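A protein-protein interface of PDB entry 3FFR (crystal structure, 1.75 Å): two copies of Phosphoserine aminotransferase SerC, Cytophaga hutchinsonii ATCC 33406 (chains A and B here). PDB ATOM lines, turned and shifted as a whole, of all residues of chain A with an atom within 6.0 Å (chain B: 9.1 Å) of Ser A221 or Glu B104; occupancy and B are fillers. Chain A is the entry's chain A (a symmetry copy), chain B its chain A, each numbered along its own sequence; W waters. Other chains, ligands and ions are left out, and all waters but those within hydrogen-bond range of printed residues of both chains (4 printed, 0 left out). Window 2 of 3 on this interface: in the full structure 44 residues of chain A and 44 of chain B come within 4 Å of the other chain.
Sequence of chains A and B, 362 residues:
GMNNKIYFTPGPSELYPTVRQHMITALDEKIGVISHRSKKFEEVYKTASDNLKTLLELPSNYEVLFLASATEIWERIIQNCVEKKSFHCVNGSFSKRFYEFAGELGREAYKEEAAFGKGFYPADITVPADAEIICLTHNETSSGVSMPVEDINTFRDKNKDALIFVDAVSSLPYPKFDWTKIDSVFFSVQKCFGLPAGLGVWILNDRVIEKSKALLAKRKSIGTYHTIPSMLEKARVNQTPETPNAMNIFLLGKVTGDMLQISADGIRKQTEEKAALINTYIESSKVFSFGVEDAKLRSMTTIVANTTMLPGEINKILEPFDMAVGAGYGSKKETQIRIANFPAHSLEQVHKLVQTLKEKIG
Gln B79 touches its own counterpart, Gln A79.
Among the printed residues, merely in contact across the chains: Gln A79 with Gln B79, Ser A221 with Leu B105, Gly A223 with Glu B104, Thr A224 with Phe B101, Thr A224 with Glu B104, Thr A224 with Leu B105, Tyr A225 with Thr B71, Tyr A225 with Glu B75 and Tyr A225 with Phe B101.
The side-chain carboxylate (OE2) of Glu B104 is in salt-bridge range of the guanidinium group (NH1) of Arg B97, at 2.8 Å.
N of Gly A223 is in hydrogen-bond range of OG of Ser A221 (3.3 Å).
O of Leu B105 lies within hydrogen-bond range of NH1 of Arg B107.
Printed residues of chain B within 4 Å of Gln A79: Gln B79 (3.96 Å).
Ser A221 touches just these residues of chain B: Glu B104 and Leu B105.
Printed residues of chain A within 4 Å of Thr B71: Tyr A225.
Trp B74 touches none of the printed residues of chain A.
Printed residues of chain A within 4 Å of Phe B101: Thr A224 (3.4 Å) and Tyr A225 (3.9 Å).
Of the printed residues of chain A, Leu B105 touches Ser A221 and Thr A224.
Water W4 bridges OE2 of Glu B75 (2.7 Å) and N of Thr A224 (2.8 Å).
Water W3 bridges the backbone carbonyl oxygen (O) of Thr A224 (2.7 Å) and the side-chain carboxylate (OE1) of Glu B104 (2.9 Å).
Water W1 lies within hydrogen-bond range of OE2 of Glu B75 (2.9 Å), NE2 of Gln B79 (3.0 Å) and NE2 of Gln A79 (3.2 Å).
Water W2 lies within hydrogen-bond range of the side-chain amide nitrogen of Gln A79 and the side-chain amide nitrogen of Gln B79.
The side-chain carboxylate (OE2) of Glu B75 sits at hydrogen-bond distance from the side-chain hydroxyl (OG1) of Thr A224, at 2.7 Å.
The backbone carbonyl oxygen (O) of Glu B104 is in hydrogen-bond range of the side-chain hydroxyl (OG) of Ser A221 (2.7 Å).
Of the 11 printed residues of chain A, 5 touch a printed residue of chain B.
Of the 19 printed residues of chain B, 6 touch a printed residue of chain A.
Among the printed residues, no Asp or Glu carboxylate lies within 4 Å of a Lys or Arg side-chain nitrogen of the other chain.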
ATOM      1  N   GLN A  79      -7.935   0.419 -41.035  1.00  0.00           N
ATOM      2  CA  GLN A  79      -7.733  -0.327 -39.774  1.00  0.00           C
ATOM      3  C   GLN A  79      -8.172  -1.757 -39.794  1.00  0.00           C
ATOM      4  O   GLN A  79      -7.521  -2.643 -39.213  1.00  0.00           O
ATOM      5  CB  GLN A  79      -8.440   0.372 -38.598  1.00  0.00           C
ATOM      6  CG  GLN A  79      -7.844   1.745 -38.266  1.00  0.00           C
ATOM      7  CD  GLN A  79      -8.706   2.554 -37.289  1.00  0.00           C
ATOM      8  OE1 GLN A  79      -9.914   2.336 -37.181  1.00  0.00           O
ATOM      9  NE2 GLN A  79      -8.082   3.488 -36.572  1.00  0.00           N
ATOM     10  N   ARG A 107       0.666   2.586 -42.653  1.00  0.00           N
ATOM     11  CA  ARG A 107       0.681   1.695 -43.805  1.00  0.00           C
ATOM     12  C   ARG A 107       1.436   2.339 -44.950  1.00  0.00           C
ATOM     13  O   ARG A 107       1.654   3.535 -44.992  1.00  0.00           O
ATOM     14  CB  ARG A 107      -0.736   1.371 -44.300  1.00  0.00           C
ATOM     15  CG  ARG A 107      -1.477   0.301 -43.551  1.00  0.00           C
ATOM     16  CD  ARG A 107      -1.666   0.543 -42.110  1.00  0.00           C
ATOM     17  NE  ARG A 107      -2.631  -0.427 -41.579  1.00  0.00           N
ATOM     18  CZ  ARG A 107      -3.127  -0.372 -40.356  1.00  0.00           C
ATOM     19  NH1 ARG A 107      -2.708   0.566 -39.531  1.00  0.00           N
ATOM     20  NH2 ARG A 107      -4.025  -1.249 -39.945  1.00  0.00           N
ATOM     21  N   LEU A 215      -7.126 -10.563 -39.900  1.00  0.00           N
ATOM     22  CA  LEU A 215      -6.151  -9.647 -39.261  1.00  0.00           C
ATOM     23  C   LEU A 215      -6.237  -9.719 -37.752  1.00  0.00           C
ATOM     24  O   LEU A 215      -5.226  -9.765 -37.057  1.00  0.00           O
ATOM     25  CB  LEU A 215      -6.382  -8.201 -39.675  1.00  0.00           C
ATOM     26  CG  LEU A 215      -5.960  -7.891 -41.083  1.00  0.00           C
ATOM     27  CD1 LEU A 215      -6.124  -6.368 -41.309  1.00  0.00           C
ATOM     28  CD2 LEU A 215      -4.505  -8.353 -41.300  1.00  0.00           C
ATOM     29  N   LEU A 216      -7.463  -9.780 -37.259  1.00  0.00           N
ATOM     30  CA  LEU A 216      -7.690  -9.879 -35.810  1.00  0.00           C
ATOM     31  C   LEU A 216      -7.072 -11.187 -35.310  1.00  0.00           C
ATOM     32  O   LEU A 216      -6.444 -11.223 -34.263  1.00  0.00           O
ATOM     33  CB  LEU A 216      -9.186  -9.814 -35.453  1.00  0.00           C
ATOM     34  CG  LEU A 216      -9.521  -9.821 -33.948  1.00  0.00           C
ATOM     35  CD1 LEU A 216      -8.899  -8.661 -33.248  1.00  0.00           C
ATOM     36  CD2 LEU A 216     -11.013  -9.845 -33.719  1.00  0.00           C
ATOM     37  N   ARG A 219      -3.566 -11.526 -34.388  1.00  0.00           N
ATOM     38  CA  ARG A 219      -3.300 -10.746 -33.165  1.00  0.00           C
ATOM     39  C   ARG A 219      -3.016  -9.273 -33.427  1.00  0.00           C
ATOM     40  O   ARG A 219      -2.324  -8.615 -32.660  1.00  0.00           O
ATOM     41  CB  ARG A 219      -2.182 -11.358 -32.325  1.00  0.00           C
ATOM     42  CG  ARG A 219      -2.552 -12.736 -31.778  1.00  0.00           C
ATOM     43  CD  ARG A 219      -1.544 -13.254 -30.727  1.00  0.00           C
ATOM     44  N   LYS A 220      -3.527  -8.789 -34.544  1.00  0.00           N
ATOM     45  CA  LYS A 220      -3.446  -7.355 -34.872  1.00  0.00           C
ATOM     46  C   LYS A 220      -4.671  -6.651 -34.303  1.00  0.00           C
ATOM     47  O   LYS A 220      -5.767  -7.179 -34.353  1.00  0.00           O
ATOM     48  CB  LYS A 220      -3.475  -7.106 -36.399  1.00  0.00           C
ATOM     49  CG  LYS A 220      -2.452  -7.857 -37.195  1.00  0.00           C
ATOM     50  CD  LYS A 220      -1.059  -7.391 -36.885  1.00  0.00           C
ATOM     51  CE  LYS A 220      -0.103  -7.813 -37.993  1.00  0.00           C
ATOM     52  NZ  LYS A 220       1.226  -7.163 -37.840  1.00  0.00           N
ATOM     53  N   SER A 221      -4.486  -5.463 -33.750  1.00  0.00           N
ATOM     54  CA  SER A 221      -5.658  -4.677 -33.335  1.00  0.00           C
ATOM     55  C   SER A 221      -6.281  -4.107 -34.586  1.00  0.00           C
ATOM     56  O   SER A 221      -5.571  -3.524 -35.423  1.00  0.00           O
ATOM     57  CB  SER A 221      -5.292  -3.525 -32.423  1.00  0.00           C
ATOM     58  OG  SER A 221      -6.441  -2.723 -32.224  1.00  0.00           O
ATOM     59  N   ILE A 222      -7.593  -4.282 -34.717  1.00  0.00           N
ATOM     60  CA  ILE A 222      -8.372  -3.729 -35.838  1.00  0.00           C
ATOM     61  C   ILE A 222      -9.338  -2.647 -35.353  1.00  0.00           C
ATOM     62  O   ILE A 222     -10.180  -2.125 -36.121  1.00  0.00           O
ATOM     63  CB  ILE A 222      -9.112  -4.780 -36.678  1.00  0.00           C
ATOM     64  CG1 ILE A 222     -10.076  -5.631 -35.819  1.00  0.00           C
ATOM     65  CG2 ILE A 222      -8.078  -5.632 -37.442  1.00  0.00           C
ATOM     66  CD1 ILE A 222     -10.972  -6.551 -36.641  1.00  0.00           C
ATOM     67  N   GLY A 223      -9.183  -2.320 -34.071  1.00  0.00           N
ATOM     68  CA  GLY A 223      -9.978  -1.274 -33.457  1.00  0.00           C
ATOM     69  C   GLY A 223     -10.689  -1.674 -32.182  1.00  0.00           C
ATOM     70  O   GLY A 223     -10.308  -2.611 -31.494  1.00  0.00           O
ATOM     71  N   THR A 224     -11.787  -0.950 -31.935  1.00  0.00           N
ATOM     72  CA  THR A 224     -12.584  -1.148 -30.721  1.00  0.00           C
ATOM     73  C   THR A 224     -14.061  -1.280 -31.076  1.00  0.00           C
ATOM     74  O   THR A 224     -14.486  -2.358 -31.504  1.00  0.00           O
ATOM     75  CB  THR A 224     -12.338  -0.069 -29.634  1.00  0.00           C
ATOM     76  OG1 THR A 224     -12.716   1.230 -30.104  1.00  0.00           O
ATOM     77  CG2 THR A 224     -10.867  -0.082 -29.130  1.00  0.00           C
ATOM     78  N   TYR A 225     -14.812  -0.211 -30.879  1.00  0.00           N
ATOM     79  CA  TYR A 225     -16.268  -0.241 -31.122  1.00  0.00           C
ATOM     80  C   TYR A 225     -16.642  -0.403 -32.569  1.00  0.00           C
ATOM     81  O   TYR A 225     -17.698  -0.979 -32.897  1.00  0.00           O
ATOM     82  CB  TYR A 225     -16.986   0.985 -30.470  1.00  0.00           C
ATOM     83  CG  TYR A 225     -16.742   2.293 -31.152  1.00  0.00           C
ATOM     84  CD1 TYR A 225     -15.479   2.870 -31.186  1.00  0.00           C
ATOM     85  CD2 TYR A 225     -17.766   2.946 -31.789  1.00  0.00           C
ATOM     86  CE1 TYR A 225     -15.246   4.060 -31.857  1.00  0.00           C
ATOM     87  CE2 TYR A 225     -17.555   4.155 -32.461  1.00  0.00           C
ATOM     88  CZ  TYR A 225     -16.290   4.694 -32.506  1.00  0.00           C
ATOM     89  OH  TYR A 225     -16.067   5.859 -33.192  1.00  0.00           O
ATOM     90  N   THR B  71     -18.416   6.942 -26.885  1.00  0.00           N
ATOM     91  CA  THR B  71     -17.674   5.695 -27.154  1.00  0.00           C
ATOM     92  C   THR B  71     -16.478   5.979 -28.087  1.00  0.00           C
ATOM     93  O   THR B  71     -15.344   5.517 -27.867  1.00  0.00           O
ATOM     94  CB  THR B  71     -18.584   4.592 -27.733  1.00  0.00           C
ATOM     95  OG1 THR B  71     -19.671   4.334 -26.825  1.00  0.00           O
ATOM     96  CG2 THR B  71     -17.815   3.264 -27.968  1.00  0.00           C
ATOM     97  N   TRP B  74     -13.798   7.471 -25.943  1.00  0.00           N
ATOM     98  CA  TRP B  74     -12.976   6.457 -25.227  1.00  0.00           C
ATOM     99  C   TRP B  74     -11.787   6.012 -26.112  1.00  0.00           C
ATOM    100  O   TRP B  74     -10.638   5.938 -25.711  1.00  0.00           O
ATOM    101  CB  TRP B  74     -13.765   5.212 -24.908  1.00  0.00           C
ATOM    102  CG  TRP B  74     -14.760   5.301 -23.815  1.00  0.00           C
ATOM    103  CD1 TRP B  74     -14.854   6.230 -22.821  1.00  0.00           C
ATOM    104  CD2 TRP B  74     -15.811   4.356 -23.576  1.00  0.00           C
ATOM    105  NE1 TRP B  74     -15.910   5.921 -21.974  1.00  0.00           N
ATOM    106  CE2 TRP B  74     -16.508   4.776 -22.421  1.00  0.00           C
ATOM    107  CE3 TRP B  74     -16.214   3.201 -24.215  1.00  0.00           C
ATOM    108  CZ2 TRP B  74     -17.565   4.043 -21.891  1.00  0.00           C
ATOM    109  CZ3 TRP B  74     -17.273   2.499 -23.714  1.00  0.00           C
ATOM    110  CH2 TRP B  74     -17.954   2.924 -22.577  1.00  0.00           C
ATOM    111  N   GLU B  75     -12.109   5.641 -27.340  1.00  0.00           N
ATOM    112  CA  GLU B  75     -11.085   5.187 -28.295  1.00  0.00           C
ATOM    113  C   GLU B  75     -10.022   6.248 -28.558  1.00  0.00           C
ATOM    114  O   GLU B  75      -8.807   5.960 -28.536  1.00  0.00           O
ATOM    115  CB  GLU B  75     -11.729   4.723 -29.604  1.00  0.00           C
ATOM    116  CG  GLU B  75     -10.720   4.131 -30.589  1.00  0.00           C
ATOM    117  CD  GLU B  75     -11.361   3.742 -31.902  1.00  0.00           C
ATOM    118  OE1 GLU B  75     -11.541   4.639 -32.735  1.00  0.00           O
ATOM    119  OE2 GLU B  75     -11.544   2.543 -32.115  1.00  0.00           O
ATOM    120  N   ILE B  78      -7.373   6.879 -25.779  1.00  0.00           N
ATOM    121  CA  ILE B  78      -6.276   5.900 -25.728  1.00  0.00           C
ATOM    122  C   ILE B  78      -5.332   6.097 -26.916  1.00  0.00           C
ATOM    123  O   ILE B  78      -4.088   6.093 -26.769  1.00  0.00           O
ATOM    124  CB  ILE B  78      -6.813   4.460 -25.606  1.00  0.00           C
ATOM    125  CG1 ILE B  78      -7.654   4.313 -24.333  1.00  0.00           C
ATOM    126  CG2 ILE B  78      -5.655   3.450 -25.559  1.00  0.00           C
ATOM    127  CD1 ILE B  78      -8.562   3.072 -24.344  1.00  0.00           C
ATOM    128  N   GLN B  79      -5.898   6.318 -28.090  1.00  0.00           N
ATOM    129  CA  GLN B  79      -5.040   6.532 -29.276  1.00  0.00           C
ATOM    130  C   GLN B  79      -4.162   7.743 -29.224  1.00  0.00           C
ATOM    131  O   GLN B  79      -3.003   7.721 -29.676  1.00  0.00           O
ATOM    132  CB  GLN B  79      -5.884   6.611 -30.561  1.00  0.00           C
ATOM    133  CG  GLN B  79      -6.589   5.292 -30.902  1.00  0.00           C
ATOM    134  CD  GLN B  79      -7.635   5.440 -32.013  1.00  0.00           C
ATOM    135  OE1 GLN B  79      -8.163   6.528 -32.245  1.00  0.00           O
ATOM    136  NE2 GLN B  79      -7.930   4.340 -32.707  1.00  0.00           N
ATOM    137  N   LYS B  96     -16.049  -0.668 -17.324  1.00  0.00           N
ATOM    138  CA  LYS B  96     -15.401  -1.919 -17.769  1.00  0.00           C
ATOM    139  C   LYS B  96     -15.067  -1.907 -19.272  1.00  0.00           C
ATOM    140  O   LYS B  96     -13.980  -2.307 -19.708  1.00  0.00           O
ATOM    141  CB  LYS B  96     -16.273  -3.123 -17.461  1.00  0.00           C
ATOM    142  CG  LYS B  96     -15.749  -4.475 -17.965  1.00  0.00           C
ATOM    143  CD  LYS B  96     -16.757  -5.577 -17.522  1.00  0.00           C
ATOM    144  CE  LYS B  96     -16.461  -6.973 -18.038  1.00  0.00           C
ATOM    145  NZ  LYS B  96     -16.921  -7.141 -19.466  1.00  0.00           N
ATOM    146  N   ARG B  97     -16.010  -1.421 -20.065  1.00  0.00           N
ATOM    147  CA  ARG B  97     -15.838  -1.405 -21.537  1.00  0.00           C
ATOM    148  C   ARG B  97     -14.671  -0.487 -21.913  1.00  0.00           C
ATOM    149  O   ARG B  97     -13.834  -0.849 -22.771  1.00  0.00           O
ATOM    150  CB  ARG B  97     -17.123  -1.010 -22.271  1.00  0.00           C
ATOM    151  CG  ARG B  97     -17.044  -1.289 -23.793  1.00  0.00           C
ATOM    152  CD  ARG B  97     -17.192  -2.785 -24.181  1.00  0.00           C
ATOM    153  NE  ARG B  97     -16.847  -2.981 -25.592  1.00  0.00           N
ATOM    154  CZ  ARG B  97     -15.671  -3.463 -25.999  1.00  0.00           C
ATOM    155  NH1 ARG B  97     -14.808  -3.920 -25.113  1.00  0.00           N
ATOM    156  NH2 ARG B  97     -15.390  -3.558 -27.304  1.00  0.00           N
ATOM    157  N   PHE B  98     -14.593   0.667 -21.244  1.00  0.00           N
ATOM    158  CA  PHE B  98     -13.492   1.650 -21.478  1.00  0.00           C
ATOM    159  C   PHE B  98     -12.167   0.997 -21.151  1.00  0.00           C
ATOM    160  O   PHE B  98     -11.217   1.043 -21.918  1.00  0.00           O
ATOM    161  CB  PHE B  98     -13.787   2.929 -20.670  1.00  0.00           C
ATOM    162  CG  PHE B  98     -12.848   4.065 -20.896  1.00  0.00           C
ATOM    163  CD1 PHE B  98     -11.990   4.105 -21.984  1.00  0.00           C
ATOM    164  CD2 PHE B  98     -12.955   5.180 -20.074  1.00  0.00           C
ATOM    165  CE1 PHE B  98     -11.164   5.207 -22.178  1.00  0.00           C
ATOM    166  CE2 PHE B  98     -12.130   6.287 -20.285  1.00  0.00           C
ATOM    167  CZ  PHE B  98     -11.260   6.291 -21.322  1.00  0.00           C
ATOM    168  N   TYR B  99     -12.121   0.313 -20.017  1.00  0.00           N
ATOM    169  CA  TYR B  99     -10.924  -0.419 -19.625  1.00  0.00           C
ATOM    170  C   TYR B  99     -10.543  -1.433 -20.700  1.00  0.00           C
ATOM    171  O   TYR B  99      -9.369  -1.568 -21.060  1.00  0.00           O
ATOM    172  CB  TYR B  99     -11.178  -1.113 -18.265  1.00  0.00           C
ATOM    173  CG  TYR B  99     -10.295  -2.309 -17.959  1.00  0.00           C
ATOM    174  CD1 TYR B  99      -8.982  -2.139 -17.572  1.00  0.00           C
ATOM    175  CD2 TYR B  99     -10.798  -3.593 -18.039  1.00  0.00           C
ATOM    176  CE1 TYR B  99      -8.186  -3.218 -17.288  1.00  0.00           C
ATOM    177  CE2 TYR B  99     -10.012  -4.678 -17.779  1.00  0.00           C
ATOM    178  CZ  TYR B  99      -8.711  -4.491 -17.385  1.00  0.00           C
ATOM    179  OH  TYR B  99      -7.927  -5.597 -17.108  1.00  0.00           O
ATOM    180  N   GLU B 100     -11.546  -2.139 -21.215  1.00  0.00           N
ATOM    181  CA  GLU B 100     -11.305  -3.166 -22.251  1.00  0.00           C
ATOM    182  C   GLU B 100     -10.754  -2.602 -23.562  1.00  0.00           C
ATOM    183  O   GLU B 100      -9.951  -3.228 -24.256  1.00  0.00           O
ATOM    184  CB  GLU B 100     -12.592  -3.954 -22.539  1.00  0.00           C
ATOM    185  CG  GLU B 100     -12.960  -4.887 -21.401  1.00  0.00           C
ATOM    186  CD  GLU B 100     -14.338  -5.504 -21.534  1.00  0.00           C
ATOM    187  OE1 GLU B 100     -15.123  -5.060 -22.389  1.00  0.00           O
ATOM    188  OE2 GLU B 100     -14.644  -6.414 -20.723  1.00  0.00           O
ATOM    189  N   PHE B 101     -11.174  -1.391 -23.882  1.00  0.00           N
ATOM    190  CA  PHE B 101     -10.659  -0.722 -25.102  1.00  0.00           C
ATOM    191  C   PHE B 101      -9.142  -0.610 -25.058  1.00  0.00           C
ATOM    192  O   PHE B 101      -8.466  -0.689 -26.086  1.00  0.00           O
ATOM    193  CB  PHE B 101     -11.231   0.704 -25.253  1.00  0.00           C
ATOM    194  CG  PHE B 101     -12.573   0.774 -25.901  1.00  0.00           C
ATOM    195  CD1 PHE B 101     -13.483  -0.282 -25.839  1.00  0.00           C
ATOM    196  CD2 PHE B 101     -12.953   1.945 -26.564  1.00  0.00           C
ATOM    197  CE1 PHE B 101     -14.734  -0.195 -26.441  1.00  0.00           C
ATOM    198  CE2 PHE B 101     -14.198   2.048 -27.144  1.00  0.00           C
ATOM    199  CZ  PHE B 101     -15.092   0.991 -27.070  1.00  0.00           C
ATOM    200  N   ALA B 102      -8.586  -0.362 -23.878  1.00  0.00           N
ATOM    201  CA  ALA B 102      -7.134  -0.178 -23.794  1.00  0.00           C
ATOM    202  C   ALA B 102      -6.418  -1.433 -24.333  1.00  0.00           C
ATOM    203  O   ALA B 102      -5.526  -1.353 -25.178  1.00  0.00           O
ATOM    204  CB  ALA B 102      -6.674   0.155 -22.334  1.00  0.00           C
ATOM    205  N   GLY B 103      -6.847  -2.596 -23.847  1.00  0.00           N
ATOM    206  CA  GLY B 103      -6.289  -3.869 -24.303  1.00  0.00           C
ATOM    207  C   GLY B 103      -6.573  -4.147 -25.769  1.00  0.00           C
ATOM    208  O   GLY B 103      -5.736  -4.668 -26.503  1.00  0.00           O
ATOM    209  N   GLU B 104      -7.768  -3.804 -26.220  1.00  0.00           N
ATOM    210  CA  GLU B 104      -8.101  -4.036 -27.636  1.00  0.00           C
ATOM    211  C   GLU B 104      -7.202  -3.223 -28.567  1.00  0.00           C
ATOM    212  O   GLU B 104      -6.968  -3.599 -29.737  1.00  0.00           O
ATOM    213  CB  GLU B 104      -9.578  -3.732 -27.906  1.00  0.00           C
ATOM    214  CG  GLU B 104     -10.434  -4.779 -27.296  1.00  0.00           C
ATOM    215  CD  GLU B 104     -11.921  -4.447 -27.234  1.00  0.00           C
ATOM    216  OE1 GLU B 104     -12.377  -3.568 -27.961  1.00  0.00           O
ATOM    217  OE2 GLU B 104     -12.622  -5.072 -26.400  1.00  0.00           O
ATOM    218  N   LEU B 105      -6.694  -2.104 -28.045  1.00  0.00           N
ATOM    219  CA  LEU B 105      -5.807  -1.205 -28.796  1.00  0.00           C
ATOM    220  C   LEU B 105      -4.327  -1.510 -28.562  1.00  0.00           C
ATOM    221  O   LEU B 105      -3.436  -0.792 -29.006  1.00  0.00           O
ATOM    222  CB  LEU B 105      -6.094   0.257 -28.464  1.00  0.00           C
ATOM    223  CG  LEU B 105      -7.438   0.790 -28.983  1.00  0.00           C
ATOM    224  CD1 LEU B 105      -7.860   2.170 -28.392  1.00  0.00           C
ATOM    225  CD2 LEU B 105      -7.421   0.881 -30.543  1.00  0.00           C
ATOM    226  N   GLY B 106      -4.092  -2.594 -27.864  1.00  0.00           N
ATOM    227  CA  GLY B 106      -2.738  -3.062 -27.655  1.00  0.00           C
ATOM    228  C   GLY B 106      -1.995  -2.455 -26.488  1.00  0.00           C
ATOM    229  O   GLY B 106      -0.791  -2.610 -26.367  1.00  0.00           O
ATOM    230  N   ARG B 107      -2.719  -1.754 -25.635  1.00  0.00           N
ATOM    231  CA  ARG B 107      -2.129  -1.165 -24.439  1.00  0.00           C
ATOM    232  C   ARG B 107      -2.325  -2.090 -23.255  1.00  0.00           C
ATOM    233  O   ARG B 107      -3.155  -2.980 -23.256  1.00  0.00           O
ATOM    234  CB  ARG B 107      -2.765   0.188 -24.090  1.00  0.00           C
ATOM    235  CG  ARG B 107      -2.265   1.378 -24.856  1.00  0.00           C
ATOM    236  CD  ARG B 107      -2.407   1.302 -26.321  1.00  0.00           C
ATOM    237  NE  ARG B 107      -2.145   2.624 -26.902  1.00  0.00           N
ATOM    238  CZ  ARG B 107      -2.344   2.918 -28.175  1.00  0.00           C
ATOM    239  NH1 ARG B 107      -2.751   1.974 -28.999  1.00  0.00           N
ATOM    240  NH2 ARG B 107      -2.130   4.136 -28.634  1.00  0.00           N
ATOM    241  N   GLU B 108      -1.569  -1.807 -22.217  1.00  0.00           N
ATOM    242  CA  GLU B 108      -1.678  -2.531 -20.948  1.00  0.00           C
ATOM    243  C   GLU B 108      -2.365  -1.621 -19.936  1.00  0.00           C
ATOM    244  O   GLU B 108      -1.886  -0.540 -19.616  1.00  0.00           O
ATOM    245  CB  GLU B 108      -0.312  -2.920 -20.421  1.00  0.00           C
ATOM    246  CG  GLU B 108       0.441  -3.873 -21.296  1.00  0.00           C
ATOM    247  CD  GLU B 108       1.837  -4.204 -20.748  1.00  0.00           C
ATOM    248  OE1 GLU B 108       2.093  -3.975 -19.553  1.00  0.00           O
ATOM    249  OE2 GLU B 108       2.671  -4.689 -21.538  1.00  0.00           O
ATOM    250  N   ALA B 109      -3.466  -2.093 -19.388  1.00  0.00           N
ATOM    251  CA  ALA B 109      -4.237  -1.293 -18.431  1.00  0.00           C
ATOM    252  C   ALA B 109      -4.267  -1.861 -17.018  1.00  0.00           C
ATOM    253  O   ALA B 109      -4.501  -3.049 -16.810  1.00  0.00           O
ATOM    254  CB  ALA B 109      -5.700  -1.144 -18.948  1.00  0.00           C
HETATM  255  O   HOH W   1      -9.395   2.133 -34.038  1.00  0.00           O
HETATM  256  O   HOH W   2      -7.339   6.058 -35.293  1.00  0.00           O
HETATM  257  O   HOH W   3     -13.526  -4.669 -30.444  1.00  0.00           O
HETATM  258  O   HOH W   4     -12.964   0.900 -33.746  1.00  0.00           O
